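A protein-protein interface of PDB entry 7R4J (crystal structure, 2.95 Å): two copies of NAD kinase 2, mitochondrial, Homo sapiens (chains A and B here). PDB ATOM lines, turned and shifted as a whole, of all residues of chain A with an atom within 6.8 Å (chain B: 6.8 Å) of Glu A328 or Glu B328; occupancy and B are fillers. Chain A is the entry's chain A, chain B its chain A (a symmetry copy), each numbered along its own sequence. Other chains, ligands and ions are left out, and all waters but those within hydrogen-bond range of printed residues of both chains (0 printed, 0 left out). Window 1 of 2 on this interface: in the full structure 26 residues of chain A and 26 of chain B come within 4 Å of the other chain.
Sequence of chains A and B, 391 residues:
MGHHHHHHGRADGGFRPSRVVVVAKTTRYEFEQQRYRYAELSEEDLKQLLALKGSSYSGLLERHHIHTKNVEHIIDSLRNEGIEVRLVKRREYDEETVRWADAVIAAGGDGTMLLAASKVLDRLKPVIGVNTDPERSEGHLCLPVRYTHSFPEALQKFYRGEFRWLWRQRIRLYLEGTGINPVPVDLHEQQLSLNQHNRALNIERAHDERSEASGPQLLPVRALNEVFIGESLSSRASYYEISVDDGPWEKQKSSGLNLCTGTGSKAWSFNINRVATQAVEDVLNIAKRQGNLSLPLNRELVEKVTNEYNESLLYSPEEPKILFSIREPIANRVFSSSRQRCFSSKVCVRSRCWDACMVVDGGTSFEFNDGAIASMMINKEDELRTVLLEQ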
ATOM      1  N   LYS A 253     -16.702  10.046  31.217  1.00  0.00           N
ATOM      2  CA  LYS A 253     -17.356  10.224  29.923  1.00  0.00           C
ATOM      3  C   LYS A 253     -17.387  11.715  29.614  1.00  0.00           C
ATOM      4  O   LYS A 253     -17.951  12.494  30.389  1.00  0.00           O
ATOM      5  CB  LYS A 253     -18.771   9.621  29.917  1.00  0.00           C
ATOM      6  CG  LYS A 253     -19.147   8.974  28.587  1.00  0.00           C
ATOM      7  CD  LYS A 253     -20.506   8.304  28.610  1.00  0.00           C
ATOM      8  CE  LYS A 253     -20.659   7.281  27.467  1.00  0.00           C
ATOM      9  NZ  LYS A 253     -19.999   5.953  27.664  1.00  0.00           N
ATOM     10  N   SER A 254     -16.754  12.118  28.511  1.00  0.00           N
ATOM     11  CA  SER A 254     -16.646  13.533  28.157  1.00  0.00           C
ATOM     12  C   SER A 254     -16.392  13.671  26.658  1.00  0.00           C
ATOM     13  O   SER A 254     -16.318  12.686  25.922  1.00  0.00           O
ATOM     14  CB  SER A 254     -15.537  14.225  28.954  1.00  0.00           C
ATOM     15  OG  SER A 254     -14.341  13.470  28.908  1.00  0.00           O
ATOM     16  N   SER A 255     -16.266  14.918  26.209  1.00  0.00           N
ATOM     17  CA  SER A 255     -15.898  15.220  24.834  1.00  0.00           C
ATOM     18  C   SER A 255     -14.381  15.251  24.630  1.00  0.00           C
ATOM     19  O   SER A 255     -13.908  15.860  23.661  1.00  0.00           O
ATOM     20  CB  SER A 255     -16.511  16.557  24.405  1.00  0.00           C
ATOM     21  OG  SER A 255     -17.856  16.671  24.837  1.00  0.00           O
ATOM     22  N   GLY A 256     -13.614  14.628  25.523  1.00  0.00           N
ATOM     23  CA  GLY A 256     -12.190  14.443  25.343  1.00  0.00           C
ATOM     24  C   GLY A 256     -11.390  14.892  26.555  1.00  0.00           C
ATOM     25  O   GLY A 256     -11.923  15.366  27.562  1.00  0.00           O
ATOM     26  N   TRP A 268      -4.929  25.824  23.916  1.00  0.00           N
ATOM     27  CA  TRP A 268      -6.234  25.182  23.964  1.00  0.00           C
ATOM     28  C   TRP A 268      -6.766  25.124  25.385  1.00  0.00           C
ATOM     29  O   TRP A 268      -7.934  25.442  25.614  1.00  0.00           O
ATOM     30  CB  TRP A 268      -6.186  23.772  23.385  1.00  0.00           C
ATOM     31  CG  TRP A 268      -7.540  23.332  22.911  1.00  0.00           C
ATOM     32  CD1 TRP A 268      -8.758  23.778  23.359  1.00  0.00           C
ATOM     33  CD2 TRP A 268      -7.824  22.326  21.936  1.00  0.00           C
ATOM     34  NE1 TRP A 268      -9.777  23.136  22.696  1.00  0.00           N
ATOM     35  CE2 TRP A 268      -9.231  22.237  21.820  1.00  0.00           C
ATOM     36  CE3 TRP A 268      -7.026  21.500  21.135  1.00  0.00           C
ATOM     37  CZ2 TRP A 268      -9.855  21.353  20.937  1.00  0.00           C
ATOM     38  CZ3 TRP A 268      -7.651  20.620  20.246  1.00  0.00           C
ATOM     39  CH2 TRP A 268      -9.050  20.554  20.162  1.00  0.00           C
ATOM     40  N   ASN A 271      -9.198  28.058  26.093  1.00  0.00           N
ATOM     41  CA  ASN A 271     -10.534  28.066  25.484  1.00  0.00           C
ATOM     42  C   ASN A 271     -11.460  27.003  26.073  1.00  0.00           C
ATOM     43  O   ASN A 271     -12.685  27.199  26.101  1.00  0.00           O
ATOM     44  CB  ASN A 271     -10.419  27.854  23.973  1.00  0.00           C
ATOM     45  CG  ASN A 271      -9.431  28.806  23.307  1.00  0.00           C
ATOM     46  OD1 ASN A 271      -9.045  29.821  23.881  1.00  0.00           O
ATOM     47  ND2 ASN A 271      -8.992  28.451  22.089  1.00  0.00           N
ATOM     48  N   ILE A 272     -10.898  25.866  26.506  1.00  0.00           N
ATOM     49  CA  ILE A 272     -11.655  24.851  27.248  1.00  0.00           C
ATOM     50  C   ILE A 272     -12.286  25.466  28.499  1.00  0.00           C
ATOM     51  O   ILE A 272     -13.502  25.360  28.724  1.00  0.00           O
ATOM     52  CB  ILE A 272     -10.734  23.672  27.641  1.00  0.00           C
ATOM     53  CG1 ILE A 272     -10.326  22.771  26.474  1.00  0.00           C
ATOM     54  CG2 ILE A 272     -11.426  22.798  28.665  1.00  0.00           C
ATOM     55  CD1 ILE A 272     -11.364  22.567  25.440  1.00  0.00           C
ATOM     56  N   ASN A 273     -11.455  26.125  29.337  1.00  0.00           N
ATOM     57  CA  ASN A 273     -11.782  26.422  30.732  1.00  0.00           C
ATOM     58  C   ASN A 273     -12.183  27.870  31.009  1.00  0.00           C
ATOM     59  O   ASN A 273     -12.796  28.137  32.060  1.00  0.00           O
ATOM     60  CB  ASN A 273     -10.596  26.072  31.631  1.00  0.00           C
ATOM     61  CG  ASN A 273     -10.229  24.617  31.550  1.00  0.00           C
ATOM     62  OD1 ASN A 273     -10.989  23.752  31.994  1.00  0.00           O
ATOM     63  ND2 ASN A 273      -9.062  24.326  30.977  1.00  0.00           N
ATOM     64  N   ARG A 274     -11.857  28.799  30.111  1.00  0.00           N
ATOM     65  CA  ARG A 274     -12.186  30.206  30.314  1.00  0.00           C
ATOM     66  C   ARG A 274     -13.691  30.419  30.500  1.00  0.00           C
ATOM     67  O   ARG A 274     -14.522  29.621  30.043  1.00  0.00           O
ATOM     68  CB  ARG A 274     -11.674  31.028  29.132  1.00  0.00           C
ATOM     69  CG  ARG A 274     -12.440  30.810  27.836  1.00  0.00           C
ATOM     70  CD  ARG A 274     -12.189  31.948  26.880  1.00  0.00           C
ATOM     71  NE  ARG A 274     -12.816  33.159  27.377  1.00  0.00           N
ATOM     72  CZ  ARG A 274     -13.575  33.943  26.632  1.00  0.00           C
ATOM     73  NH1 ARG A 274     -13.802  33.669  25.356  1.00  0.00           N
ATOM     74  NH2 ARG A 274     -14.126  35.023  27.180  1.00  0.00           N
ATOM     75  N   ILE A 326     -10.792  18.112  31.883  1.00  0.00           N
ATOM     76  CA  ILE A 326     -11.728  17.217  31.222  1.00  0.00           C
ATOM     77  C   ILE A 326     -12.629  18.099  30.385  1.00  0.00           C
ATOM     78  O   ILE A 326     -13.311  18.974  30.933  1.00  0.00           O
ATOM     79  CB  ILE A 326     -12.532  16.410  32.252  1.00  0.00           C
ATOM     80  CG1 ILE A 326     -11.575  15.614  33.135  1.00  0.00           C
ATOM     81  CG2 ILE A 326     -13.541  15.511  31.571  1.00  0.00           C
ATOM     82  CD1 ILE A 326     -12.156  14.369  33.733  1.00  0.00           C
ATOM     83  N   ARG A 327     -12.627  17.915  29.066  1.00  0.00           N
ATOM     84  CA  ARG A 327     -13.384  18.821  28.196  1.00  0.00           C
ATOM     85  C   ARG A 327     -14.869  18.461  28.202  1.00  0.00           C
ATOM     86  O   ARG A 327     -15.234  17.338  27.840  1.00  0.00           O
ATOM     87  CB  ARG A 327     -12.849  18.789  26.766  1.00  0.00           C
ATOM     88  CG  ARG A 327     -13.684  19.608  25.781  1.00  0.00           C
ATOM     89  CD  ARG A 327     -13.458  19.154  24.355  1.00  0.00           C
ATOM     90  NE  ARG A 327     -13.713  20.211  23.386  1.00  0.00           N
ATOM     91  CZ  ARG A 327     -13.553  20.072  22.076  1.00  0.00           C
ATOM     92  NH1 ARG A 327     -13.182  18.917  21.542  1.00  0.00           N
ATOM     93  NH2 ARG A 327     -13.764  21.120  21.282  1.00  0.00           N
ATOM     94  N   GLU A 328     -15.718  19.420  28.584  1.00  0.00           N
ATOM     95  CA  GLU A 328     -17.166  19.259  28.730  1.00  0.00           C
ATOM     96  C   GLU A 328     -17.553  17.913  29.364  1.00  0.00           C
ATOM     97  O   GLU A 328     -18.230  17.102  28.713  1.00  0.00           O
ATOM     98  CB  GLU A 328     -17.878  19.451  27.399  1.00  0.00           C
ATOM     99  CG  GLU A 328     -17.337  20.536  26.538  1.00  0.00           C
ATOM    100  CD  GLU A 328     -17.889  20.453  25.124  1.00  0.00           C
ATOM    101  OE1 GLU A 328     -17.712  21.431  24.354  1.00  0.00           O
ATOM    102  OE2 GLU A 328     -18.497  19.406  24.784  1.00  0.00           O
ATOM    103  N   PRO A 329     -17.180  17.668  30.622  1.00  0.00           N
ATOM    104  CA  PRO A 329     -17.490  16.373  31.236  1.00  0.00           C
ATOM    105  C   PRO A 329     -18.987  16.120  31.252  1.00  0.00           C
ATOM    106  O   PRO A 329     -19.796  17.052  31.305  1.00  0.00           O
ATOM    107  CB  PRO A 329     -16.928  16.508  32.654  1.00  0.00           C
ATOM    108  CG  PRO A 329     -16.900  17.975  32.903  1.00  0.00           C
ATOM    109  CD  PRO A 329     -16.582  18.606  31.591  1.00  0.00           C
ATOM    110  N   ILE A 330     -19.349  14.840  31.188  1.00  0.00           N
ATOM    111  CA  ILE A 330     -20.742  14.408  31.187  1.00  0.00           C
ATOM    112  C   ILE A 330     -20.971  13.648  32.488  1.00  0.00           C
ATOM    113  O   ILE A 330     -20.598  12.474  32.618  1.00  0.00           O
ATOM    114  CB  ILE A 330     -21.077  13.549  29.963  1.00  0.00           C
ATOM    115  CG1 ILE A 330     -20.712  14.304  28.672  1.00  0.00           C
ATOM    116  CG2 ILE A 330     -22.561  13.146  29.998  1.00  0.00           C
ATOM    117  CD1 ILE A 330     -21.141  13.629  27.379  1.00  0.00           C
ATOM    118  N   ALA A 331     -21.586  14.323  33.453  1.00  0.00           N
ATOM    119  CA  ALA A 331     -21.875  13.745  34.760  1.00  0.00           C
ATOM    120  C   ALA A 331     -23.123  12.861  34.714  1.00  0.00           C
ATOM    121  O   ALA A 331     -23.112  11.716  35.181  1.00  0.00           O
ATOM    122  CB  ALA A 331     -22.043  14.852  35.800  1.00  0.00           C
ATOM    123  N   LYS B 253     -14.758  32.804  15.301  1.00  0.00           N
ATOM    124  CA  LYS B 253     -13.762  31.737  15.366  1.00  0.00           C
ATOM    125  C   LYS B 253     -14.002  30.949  16.647  1.00  0.00           C
ATOM    126  O   LYS B 253     -13.957  31.522  17.741  1.00  0.00           O
ATOM    127  CB  LYS B 253     -12.330  32.297  15.312  1.00  0.00           C
ATOM    128  CG  LYS B 253     -11.365  31.414  14.526  1.00  0.00           C
ATOM    129  CD  LYS B 253      -9.978  32.009  14.399  1.00  0.00           C
ATOM    130  CE  LYS B 253      -9.184  31.369  13.242  1.00  0.00           C
ATOM    131  NZ  LYS B 253      -9.515  31.840  11.861  1.00  0.00           N
ATOM    132  N   SER B 254     -14.291  29.654  16.515  1.00  0.00           N
ATOM    133  CA  SER B 254     -14.621  28.816  17.669  1.00  0.00           C
ATOM    134  C   SER B 254     -14.364  27.350  17.331  1.00  0.00           C
ATOM    135  O   SER B 254     -13.927  27.008  16.231  1.00  0.00           O
ATOM    136  CB  SER B 254     -16.075  29.018  18.108  1.00  0.00           C
ATOM    137  OG  SER B 254     -16.949  28.937  16.998  1.00  0.00           O
ATOM    138  N   SER B 255     -14.635  26.481  18.302  1.00  0.00           N
ATOM    139  CA  SER B 255     -14.566  25.041  18.104  1.00  0.00           C
ATOM    140  C   SER B 255     -15.872  24.464  17.552  1.00  0.00           C
ATOM    141  O   SER B 255     -16.115  23.258  17.697  1.00  0.00           O
ATOM    142  CB  SER B 255     -14.198  24.344  19.417  1.00  0.00           C
ATOM    143  OG  SER B 255     -13.163  25.033  20.097  1.00  0.00           O
ATOM    144  N   GLY B 256     -16.719  25.294  16.946  1.00  0.00           N
ATOM    145  CA  GLY B 256     -17.896  24.838  16.238  1.00  0.00           C
ATOM    146  C   GLY B 256     -19.153  25.576  16.669  1.00  0.00           C
ATOM    147  O   GLY B 256     -19.141  26.455  17.534  1.00  0.00           O
ATOM    148  N   TRP B 268     -26.820  17.777  23.641  1.00  0.00           N
ATOM    149  CA  TRP B 268     -25.497  18.372  23.527  1.00  0.00           C
ATOM    150  C   TRP B 268     -25.496  19.810  24.015  1.00  0.00           C
ATOM    151  O   TRP B 268     -24.600  20.200  24.766  1.00  0.00           O
ATOM    152  CB  TRP B 268     -24.984  18.325  22.091  1.00  0.00           C
ATOM    153  CG  TRP B 268     -23.486  18.390  22.047  1.00  0.00           C
ATOM    154  CD1 TRP B 268     -22.653  18.947  22.985  1.00  0.00           C
ATOM    155  CD2 TRP B 268     -22.637  17.929  20.993  1.00  0.00           C
ATOM    156  NE1 TRP B 268     -21.341  18.826  22.594  1.00  0.00           N
ATOM    157  CE2 TRP B 268     -21.304  18.209  21.372  1.00  0.00           C
ATOM    158  CE3 TRP B 268     -22.871  17.291  19.769  1.00  0.00           C
ATOM    159  CZ2 TRP B 268     -20.210  17.873  20.570  1.00  0.00           C
ATOM    160  CZ3 TRP B 268     -21.777  16.949  18.969  1.00  0.00           C
ATOM    161  CH2 TRP B 268     -20.467  17.248  19.375  1.00  0.00           C
ATOM    162  N   ASN B 271     -24.284  20.045  27.689  1.00  0.00           N
ATOM    163  CA  ASN B 271     -22.867  19.828  28.009  1.00  0.00           C
ATOM    164  C   ASN B 271     -21.968  20.961  27.517  1.00  0.00           C
ATOM    165  O   ASN B 271     -20.921  21.226  28.127  1.00  0.00           O
ATOM    166  CB  ASN B 271     -22.392  18.507  27.400  1.00  0.00           C
ATOM    167  CG  ASN B 271     -23.292  17.326  27.750  1.00  0.00           C
ATOM    168  OD1 ASN B 271     -24.096  17.396  28.677  1.00  0.00           O
ATOM    169  ND2 ASN B 271     -23.176  16.238  26.973  1.00  0.00           N
ATOM    170  N   ILE B 272     -22.341  21.605  26.402  1.00  0.00           N
ATOM    171  CA  ILE B 272     -21.660  22.817  25.934  1.00  0.00           C
ATOM    172  C   ILE B 272     -21.680  23.894  27.022  1.00  0.00           C
ATOM    173  O   ILE B 272     -20.633  24.440  27.405  1.00  0.00           O
ATOM    174  CB  ILE B 272     -22.332  23.349  24.646  1.00  0.00           C
ATOM    175  CG1 ILE B 272     -22.068  22.505  23.398  1.00  0.00           C
ATOM    176  CG2 ILE B 272     -21.843  24.752  24.353  1.00  0.00           C
ATOM    177  CD1 ILE B 272     -20.719  21.902  23.317  1.00  0.00           C
ATOM    178  N   ASN B 273     -22.887  24.213  27.537  1.00  0.00           N
ATOM    179  CA  ASN B 273     -23.152  25.454  28.267  1.00  0.00           C
ATOM    180  C   ASN B 273     -23.250  25.303  29.784  1.00  0.00           C
ATOM    181  O   ASN B 273     -23.130  26.315  30.501  1.00  0.00           O
ATOM    182  CB  ASN B 273     -24.448  26.090  27.763  1.00  0.00           C
ATOM    183  CG  ASN B 273     -24.385  26.428  26.300  1.00  0.00           C
ATOM    184  OD1 ASN B 273     -23.635  27.320  25.894  1.00  0.00           O
ATOM    185  ND2 ASN B 273     -25.167  25.717  25.489  1.00  0.00           N
ATOM    186  N   ARG B 274     -23.465  24.088  30.287  1.00  0.00           N
ATOM    187  CA  ARG B 274     -23.594  23.866  31.724  1.00  0.00           C
ATOM    188  C   ARG B 274     -22.353  24.339  32.485  1.00  0.00           C
ATOM    189  O   ARG B 274     -21.243  24.412  31.939  1.00  0.00           O
ATOM    190  CB  ARG B 274     -23.852  22.385  31.993  1.00  0.00           C
ATOM    191  CG  ARG B 274     -22.654  21.482  31.739  1.00  0.00           C
ATOM    192  CD  ARG B 274     -22.834  20.160  32.441  1.00  0.00           C
ATOM    193  NE  ARG B 274     -22.746  20.348  33.878  1.00  0.00           N
ATOM    194  CZ  ARG B 274     -21.998  19.594  34.664  1.00  0.00           C
ATOM    195  NH1 ARG B 274     -21.281  18.592  34.177  1.00  0.00           N
ATOM    196  NH2 ARG B 274     -21.963  19.853  35.969  1.00  0.00           N
ATOM    197  N   ILE B 326     -22.357  29.125  20.701  1.00  0.00           N
ATOM    198  CA  ILE B 326     -21.056  29.073  20.053  1.00  0.00           C
ATOM    199  C   ILE B 326     -20.173  28.237  20.955  1.00  0.00           C
ATOM    200  O   ILE B 326     -19.968  28.601  22.118  1.00  0.00           O
ATOM    201  CB  ILE B 326     -20.486  30.485  19.860  1.00  0.00           C
ATOM    202  CG1 ILE B 326     -21.456  31.318  19.028  1.00  0.00           C
ATOM    203  CG2 ILE B 326     -19.110  30.435  19.228  1.00  0.00           C
ATOM    204  CD1 ILE B 326     -20.826  32.436  18.255  1.00  0.00           C
ATOM    205  N   ARG B 327     -19.669  27.108  20.458  1.00  0.00           N
ATOM    206  CA  ARG B 327     -18.911  26.199  21.323  1.00  0.00           C
ATOM    207  C   ARG B 327     -17.482  26.703  21.515  1.00  0.00           C
ATOM    208  O   ARG B 327     -16.743  26.856  20.537  1.00  0.00           O
ATOM    209  CB  ARG B 327     -18.889  24.783  20.751  1.00  0.00           C
ATOM    210  CG  ARG B 327     -17.998  23.818  21.535  1.00  0.00           C
ATOM    211  CD  ARG B 327     -17.592  22.631  20.690  1.00  0.00           C
ATOM    212  NE  ARG B 327     -17.291  21.453  21.492  1.00  0.00           N
ATOM    213  CZ  ARG B 327     -16.944  20.277  20.984  1.00  0.00           C
ATOM    214  NH1 ARG B 327     -16.803  20.102  19.677  1.00  0.00           N
ATOM    215  NH2 ARG B 327     -16.742  19.249  21.806  1.00  0.00           N
ATOM    216  N   GLU B 328     -17.089  26.929  22.773  1.00  0.00           N
ATOM    217  CA  GLU B 328     -15.792  27.481  23.168  1.00  0.00           C
ATOM    218  C   GLU B 328     -15.324  28.617  22.244  1.00  0.00           C
ATOM    219  O   GLU B 328     -14.282  28.481  21.584  1.00  0.00           O
ATOM    220  CB  GLU B 328     -14.733  26.390  23.256  1.00  0.00           C
ATOM    221  CG  GLU B 328     -15.196  25.100  23.834  1.00  0.00           C
ATOM    222  CD  GLU B 328     -14.184  23.990  23.598  1.00  0.00           C
ATOM    223  OE1 GLU B 328     -14.323  22.910  24.227  1.00  0.00           O
ATOM    224  OE2 GLU B 328     -13.253  24.198  22.778  1.00  0.00           O
ATOM    225  N   PRO B 329     -16.037  29.745  22.207  1.00  0.00           N
ATOM    226  CA  PRO B 329     -15.644  30.827  21.297  1.00  0.00           C
ATOM    227  C   PRO B 329     -14.234  31.305  21.594  1.00  0.00           C
ATOM    228  O   PRO B 329     -13.756  31.234  22.730  1.00  0.00           O
ATOM    229  CB  PRO B 329     -16.679  31.921  21.579  1.00  0.00           C
ATOM    230  CG  PRO B 329     -17.160  31.631  22.956  1.00  0.00           C
ATOM    231  CD  PRO B 329     -17.150  30.146  23.088  1.00  0.00           C
ATOM    232  N   ILE B 330     -13.563  31.782  20.547  1.00  0.00           N
ATOM    233  CA  ILE B 330     -12.196  32.282  20.640  1.00  0.00           C
ATOM    234  C   ILE B 330     -12.250  33.778  20.358  1.00  0.00           C
ATOM    235  O   ILE B 330     -12.337  34.209  19.200  1.00  0.00           O
ATOM    236  CB  ILE B 330     -11.251  31.557  19.676  1.00  0.00           C
ATOM    237  CG1 ILE B 330     -11.322  30.038  19.909  1.00  0.00           C
ATOM    238  CG2 ILE B 330      -9.821  32.102  19.836  1.00  0.00           C
ATOM    239  CD1 ILE B 330     -10.315  29.211  19.125  1.00  0.00           C
ATOM    240  N   ALA B 331     -12.201  34.571  21.424  1.00  0.00           N
ATOM    241  CA  ALA B 331     -12.249  36.026  21.327  1.00  0.00           C
ATOM    242  C   ALA B 331     -10.883  36.604  20.951  1.00  0.00           C
ATOM    243  O   ALA B 331     -10.767  37.420  20.030  1.00  0.00           O
ATOM    244  CB  ALA B 331     -12.737  36.624  22.646  1.00  0.00           C
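The guanidinium group of Arg A327 lies within salt-bridge range of the side-chain carboxylate of Glu B328, 2.9 Å away. The guanidinium group of Arg B327 is in salt-bridge range of the side-chain carboxylate of Glu A328 (2.9 Å).
The backbone carbonyl oxygen (O) of Arg A327 is in hydrogen-bond range of the backbone NH (N) of Ser A255 (3.1 Å). The backbone NH of Ser B255 lies within hydrogen-bond range of the backbone carbonyl oxygen of Arg B327 (3.1 Å). O of Gly A256 sits at hydrogen-bond distance from N of Arg A327, 3.0 Å away. OG of Ser A255 lies within hydrogen-bond range of OE2 of Glu A328, at 2.8 Å. The backbone carbonyl oxygen (O) of Lys A253 lies within hydrogen-bond range of the backbone NH (N) of Ile A330. The side-chain carboxylate (OE2) of Glu B328 sits at hydrogen-bond distance from the side-chain hydroxyl (OG) of Ser B255, at 2.8 Å.
Among the printed residues, pairs that only touch across the chains: Ser A255 with Arg B327, Trp A268 with Glu B328, Asn A271 with Glu B328, Asn A271 with Ile B330, Ile A272 with Glu B328, Arg A274 with Pro B329, Arg A327 with Ser B255, Arg A327 with Arg B327, Glu A328 with Trp B268, Glu A328 with Asn B271, Glu A328 with Ile B272, Glu A328 with Glu B328, Pro A329 with Arg B274 and Ile A330 with Asn B271.
Of the printed residues of chain B, Glu A328 touches Trp B268 (3.6 Å), Asn B271 (3.6 Å), Ile B272 (3.2 Å), Arg B327 (2.9 Å) and Glu B328 (3.7 Å). Glu B328 touches just these residues of chain A: Trp A268, Asn A271, Ile A272, Arg A327 and Glu A328. Printed residues of chain B within 4 Å of Ile A330: Asn B271 (3.3 Å). Printed residues of chain A within 4 Å of Pro B329: Arg A274 (3.6 Å). Printed residues of chain A within 4 Å of Arg B274: Pro A329 (3.6 Å). Asn B273 touches none of the printed residues of chain A. The nearest printed residue of chain A that does not touch Ile B272 is Ser A255 (6.2 Å).
Hydrophobic or aromatic side chains of chain B within 4 Å of the printed part of chain A: Trp B268, Ile B272 and Ile B330.
Ser A255 touches Arg B327, and with the chains exchanged Arg A327 touches Ser B255. Arg A274 touches Pro B329, and with the chains exchanged Pro A329 touches Arg B274. Arg A327 touches Glu B328, and with the chains exchanged Glu A328 touches Arg B327. Glu B328 touches its own counterpart, Glu A328. Positions printed for both chains: 253, 254, 255, 256, 268, 271, 272, 273, 274, 326, 327, 328, 329, 330 and 331. Of the 16 pairs that touch across the chains among the printed residues, 16 have their exchanged pair printed and touching as well.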
